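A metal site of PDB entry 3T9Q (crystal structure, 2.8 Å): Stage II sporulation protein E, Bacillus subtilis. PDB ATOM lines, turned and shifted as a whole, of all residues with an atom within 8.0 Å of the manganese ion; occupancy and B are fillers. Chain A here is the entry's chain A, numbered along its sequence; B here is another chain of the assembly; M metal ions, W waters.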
ATOM      1  N   THR A  94     -27.119   3.602 -19.235  1.00  0.00           N
ATOM      2  CA  THR A  94     -28.447   3.255 -18.890  1.00  0.00           C
ATOM      3  C   THR A  94     -29.212   4.358 -19.567  1.00  0.00           C
ATOM      4  O   THR A  94     -28.668   5.442 -19.839  1.00  0.00           O
ATOM      5  CB  THR A  94     -28.628   3.281 -17.366  1.00  0.00           C
ATOM      6  OG1 THR A  94     -28.492   4.621 -16.865  1.00  0.00           O
ATOM      7  CG2 THR A  94     -27.571   2.415 -16.707  1.00  0.00           C
ATOM      8  N   THR A 115     -32.786   2.683 -13.050  1.00  0.00           N
ATOM      9  CA  THR A 115     -33.437   2.474 -11.802  1.00  0.00           C
ATOM     10  C   THR A 115     -34.897   2.800 -11.979  1.00  0.00           C
ATOM     11  O   THR A 115     -35.294   3.436 -12.916  1.00  0.00           O
ATOM     12  CB  THR A 115     -32.894   3.434 -10.791  1.00  0.00           C
ATOM     13  OG1 THR A 115     -33.548   4.694 -10.971  1.00  0.00           O
ATOM     14  CG2 THR A 115     -31.390   3.598 -10.945  1.00  0.00           C
ATOM     15  N   SER A 160     -31.186   8.989 -11.405  1.00  0.00           N
ATOM     16  CA  SER A 160     -30.050   8.021 -11.509  1.00  0.00           C
ATOM     17  C   SER A 160     -29.876   7.204 -10.230  1.00  0.00           C
ATOM     18  O   SER A 160     -30.528   7.500  -9.172  1.00  0.00           O
ATOM     19  CB  SER A 160     -28.730   8.696 -11.783  1.00  0.00           C
ATOM     20  OG  SER A 160     -28.669   9.895 -11.062  1.00  0.00           O
ATOM     21  N   ASP A 161     -28.973   6.208 -10.289  1.00  0.00           N
ATOM     22  CA  ASP A 161     -28.814   5.263  -9.159  1.00  0.00           C
ATOM     23  C   ASP A 161     -28.076   5.961  -8.051  1.00  0.00           C
ATOM     24  O   ASP A 161     -28.096   5.569  -6.903  1.00  0.00           O
ATOM     25  CB  ASP A 161     -28.187   3.925  -9.579  1.00  0.00           C
ATOM     26  CG  ASP A 161     -26.817   4.070 -10.226  1.00  0.00           C
ATOM     27  OD1 ASP A 161     -26.163   5.140 -10.076  1.00  0.00           O
ATOM     28  OD2 ASP A 161     -26.369   3.109 -10.889  1.00  0.00           O
ATOM     29  N   GLY A 162     -27.452   7.050  -8.416  1.00  0.00           N
ATOM     30  CA  GLY A 162     -26.749   7.827  -7.477  1.00  0.00           C
ATOM     31  C   GLY A 162     -27.713   8.308  -6.452  1.00  0.00           C
ATOM     32  O   GLY A 162     -27.387   8.292  -5.285  1.00  0.00           O
ATOM     33  N   ILE A 163     -28.864   8.803  -6.881  1.00  0.00           N
ATOM     34  CA  ILE A 163     -29.932   9.165  -5.966  1.00  0.00           C
ATOM     35  C   ILE A 163     -30.646   7.910  -5.387  1.00  0.00           C
ATOM     36  O   ILE A 163     -30.820   7.768  -4.179  1.00  0.00           O
ATOM     37  CB  ILE A 163     -30.953  10.090  -6.668  1.00  0.00           C
ATOM     38  CG1 ILE A 163     -30.475  11.515  -6.634  1.00  0.00           C
ATOM     39  CG2 ILE A 163     -32.385  10.026  -5.988  1.00  0.00           C
ATOM     40  CD1 ILE A 163     -31.314  12.430  -5.739  1.00  0.00           C
ATOM     41  N   GLU A 165     -30.004   4.750  -5.191  1.00  0.00           N
ATOM     42  CA  GLU A 165     -29.176   3.868  -4.387  1.00  0.00           C
ATOM     43  C   GLU A 165     -28.288   4.648  -3.382  1.00  0.00           C
ATOM     44  O   GLU A 165     -27.549   4.066  -2.607  1.00  0.00           O
ATOM     45  CB  GLU A 165     -28.354   2.979  -5.286  1.00  0.00           C
ATOM     46  CG  GLU A 165     -29.159   1.868  -5.856  1.00  0.00           C
ATOM     47  CD  GLU A 165     -28.438   1.113  -6.957  1.00  0.00           C
ATOM     48  OE1 GLU A 165     -27.231   1.400  -7.206  1.00  0.00           O
ATOM     49  OE2 GLU A 165     -29.067   0.224  -7.576  1.00  0.00           O
ATOM     50  N   GLU A 209     -21.286   9.653  -2.933  1.00  0.00           N
ATOM     51  CA  GLU A 209     -20.673   8.417  -3.473  1.00  0.00           C
ATOM     52  C   GLU A 209     -20.658   8.369  -5.003  1.00  0.00           C
ATOM     53  O   GLU A 209     -19.784   7.741  -5.585  1.00  0.00           O
ATOM     54  CB  GLU A 209     -21.372   7.150  -2.939  1.00  0.00           C
ATOM     55  CG  GLU A 209     -20.560   6.356  -1.892  1.00  0.00           C
ATOM     56  CD  GLU A 209     -20.767   4.790  -1.950  1.00  0.00           C
ATOM     57  OE1 GLU A 209     -19.760   4.043  -1.827  1.00  0.00           O
ATOM     58  OE2 GLU A 209     -21.926   4.317  -2.123  1.00  0.00           O
ATOM     59  N   ASP A 210     -21.646   9.021  -5.618  1.00  0.00           N
ATOM     60  CA  ASP A 210     -21.920   8.921  -7.062  1.00  0.00           C
ATOM     61  C   ASP A 210     -22.516  10.203  -7.596  1.00  0.00           C
ATOM     62  O   ASP A 210     -22.861  11.114  -6.820  1.00  0.00           O
ATOM     63  CB  ASP A 210     -22.883   7.752  -7.355  1.00  0.00           C
ATOM     64  CG  ASP A 210     -22.847   7.304  -8.840  1.00  0.00           C
ATOM     65  OD1 ASP A 210     -22.377   8.095  -9.720  1.00  0.00           O
ATOM     66  OD2 ASP A 210     -23.284   6.160  -9.110  1.00  0.00           O
ATOM     67  N   ASP A 211     -22.650  10.276  -8.924  1.00  0.00           N
ATOM     68  CA  ASP A 211     -23.369  11.389  -9.548  1.00  0.00           C
ATOM     69  C   ASP A 211     -24.793  11.176  -9.270  1.00  0.00           C
ATOM     70  O   ASP A 211     -25.291  10.038  -9.270  1.00  0.00           O
ATOM     71  CB  ASP A 211     -23.159  11.400 -11.024  1.00  0.00           C
ATOM     72  CG  ASP A 211     -21.765  11.770 -11.389  1.00  0.00           C
ATOM     73  OD1 ASP A 211     -21.351  12.911 -11.045  1.00  0.00           O
ATOM     74  OD2 ASP A 211     -21.070  10.929 -12.015  1.00  0.00           O
ATOM     75  N   MET A 212     -25.471  12.269  -9.002  1.00  0.00           N
ATOM     76  CA  MET A 212     -26.822  12.192  -8.567  1.00  0.00           C
ATOM     77  C   MET A 212     -27.668  13.064  -9.441  1.00  0.00           C
ATOM     78  O   MET A 212     -27.429  14.288  -9.572  1.00  0.00           O
ATOM     79  CB  MET A 212     -26.895  12.609  -7.109  1.00  0.00           C
ATOM     80  CG  MET A 212     -26.362  11.517  -6.135  1.00  0.00           C
ATOM     81  SD  MET A 212     -26.370  12.036  -4.407  1.00  0.00           S
ATOM     82  CE  MET A 212     -26.439  13.806  -4.571  1.00  0.00           C
ATOM     83  N   THR A 213     -28.683  12.456 -10.023  1.00  0.00           N
ATOM     84  CA  THR A 213     -29.665  13.201 -10.811  1.00  0.00           C
ATOM     85  C   THR A 213     -31.088  12.832 -10.443  1.00  0.00           C
ATOM     86  O   THR A 213     -31.437  11.636 -10.427  1.00  0.00           O
ATOM     87  CB  THR A 213     -29.425  12.910 -12.344  1.00  0.00           C
ATOM     88  OG1 THR A 213     -28.018  13.122 -12.663  1.00  0.00           O
ATOM     89  CG2 THR A 213     -30.320  13.776 -13.206  1.00  0.00           C
ATOM     90  N   LYS B  17     -20.303  13.517  -8.572  1.00  0.00           N
ATOM     91  CA  LYS B  17     -19.512  12.743  -7.600  1.00  0.00           C
ATOM     92  C   LYS B  17     -18.409  13.588  -6.971  1.00  0.00           C
ATOM     93  O   LYS B  17     -17.889  14.569  -7.575  1.00  0.00           O
ATOM     94  CB  LYS B  17     -18.859  11.567  -8.298  1.00  0.00           C
ATOM     95  CG  LYS B  17     -18.395  10.460  -7.397  1.00  0.00           C
ATOM     96  CD  LYS B  17     -17.903   9.297  -8.240  1.00  0.00           C
ATOM     97  CE  LYS B  17     -17.413   8.149  -7.372  1.00  0.00           C
ATOM     98  NZ  LYS B  17     -16.363   8.538  -6.380  1.00  0.00           N
ATOM     99  N   SER B  23     -19.739  15.006 -14.508  1.00  0.00           N
ATOM    100  CA  SER B  23     -20.518  13.823 -14.138  1.00  0.00           C
ATOM    101  C   SER B  23     -20.738  12.881 -15.325  1.00  0.00           C
ATOM    102  O   SER B  23     -20.792  13.334 -16.482  1.00  0.00           O
ATOM    103  CB  SER B  23     -21.849  14.291 -13.572  1.00  0.00           C
ATOM    104  OG  SER B  23     -22.780  13.227 -13.528  1.00  0.00           O
ATOM    105  N   GLY B  24     -20.848  11.580 -15.042  1.00  0.00           N
ATOM    106  CA  GLY B  24     -21.227  10.544 -16.018  1.00  0.00           C
ATOM    107  C   GLY B  24     -22.753  10.475 -16.162  1.00  0.00           C
ATOM    108  O   GLY B  24     -23.281   9.652 -16.902  1.00  0.00           O
ATOM    109  N   ASP B  25     -23.469  11.355 -15.461  1.00  0.00           N
ATOM    110  CA  ASP B  25     -24.910  11.460 -15.582  1.00  0.00           C
ATOM    111  C   ASP B  25     -25.205  12.579 -16.573  1.00  0.00           C
ATOM    112  O   ASP B  25     -24.656  13.631 -16.484  1.00  0.00           O
ATOM    113  CB  ASP B  25     -25.563  11.899 -14.252  1.00  0.00           C
ATOM    114  CG  ASP B  25     -25.954  10.737 -13.310  1.00  0.00           C
ATOM    115  OD1 ASP B  25     -25.664   9.534 -13.550  1.00  0.00           O
ATOM    116  OD2 ASP B  25     -26.573  11.087 -12.274  1.00  0.00           O
ATOM    117  N   SER B  42     -29.452   9.704 -18.349  1.00  0.00           N
ATOM    118  CA  SER B  42     -28.454   8.698 -18.640  1.00  0.00           C
ATOM    119  C   SER B  42     -27.242   8.725 -17.716  1.00  0.00           C
ATOM    120  O   SER B  42     -26.944   9.757 -17.081  1.00  0.00           O
ATOM    121  CB  SER B  42     -28.030   8.840 -20.074  1.00  0.00           C
ATOM    122  OG  SER B  42     -28.717   7.841 -20.751  1.00  0.00           O
ATOM    123  N   ASP B  43     -26.547   7.589 -17.696  1.00  0.00           N
ATOM    124  CA  ASP B  43     -25.470   7.314 -16.747  1.00  0.00           C
ATOM    125  C   ASP B  43     -24.489   6.490 -17.553  1.00  0.00           C
ATOM    126  O   ASP B  43     -24.791   5.366 -17.908  1.00  0.00           O
ATOM    127  CB  ASP B  43     -26.053   6.519 -15.549  1.00  0.00           C
ATOM    128  CG  ASP B  43     -25.068   6.229 -14.427  1.00  0.00           C
ATOM    129  OD1 ASP B  43     -23.921   6.728 -14.451  1.00  0.00           O
ATOM    130  OD2 ASP B  43     -25.440   5.476 -13.484  1.00  0.00           O
ATOM    131  N   GLY B  44     -23.334   7.076 -17.907  1.00  0.00           N
ATOM    132  CA  GLY B  44     -22.235   6.340 -18.563  1.00  0.00           C
ATOM    133  C   GLY B  44     -21.070   7.204 -19.023  1.00  0.00           C
ATOM    134  O   GLY B  44     -21.197   8.014 -19.965  1.00  0.00           O
HETATM  135 MN    MN M   1     -24.512   6.257 -11.265  1.00  0.00          MN
HETATM  136  O   HOH W   1     -22.309   6.354 -12.162  1.00  0.00           O
HETATM  137  O   HOH W   2     -24.004   4.120 -11.271  1.00  0.00           O
HETATM  138  O   HOH W   3     -25.368   8.532 -10.927  1.00  0.00           O
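The manganese ion is bound by water W2 (2.2 Å), the side-chain carboxylate of Asp 161 (2.3 Å), water W1 (2.4 Å), water W3 (2.5 Å), the side-chain carboxylate of Asp 210 (2.5 Å) and the side-chain carboxylate of Asp 43 of chain B (2.5 Å).
The backbone NH (N) of Thr 94 lies within hydrogen-bond range of the backbone carbonyl oxygen (O) of Asp 43 of chain B, at 3.2 Å.
Three residues have an atom within 4 Å of the manganese ion: Asp 161, Asp 210 and Asp 43 of chain B.
The nearest printed residue that does not touch the manganese ion is Asp 25 of chain B (4.2 Å).
Water W1 lies within hydrogen-bond range of the side-chain carboxylate of Asp 43 of chain B and the side-chain carboxylate of Asp 210.
Water W3 lies within hydrogen-bond range of OD1 of Asp 25 of chain B (2.8 Å) and OD1 of Asp 210 (3.3 Å).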
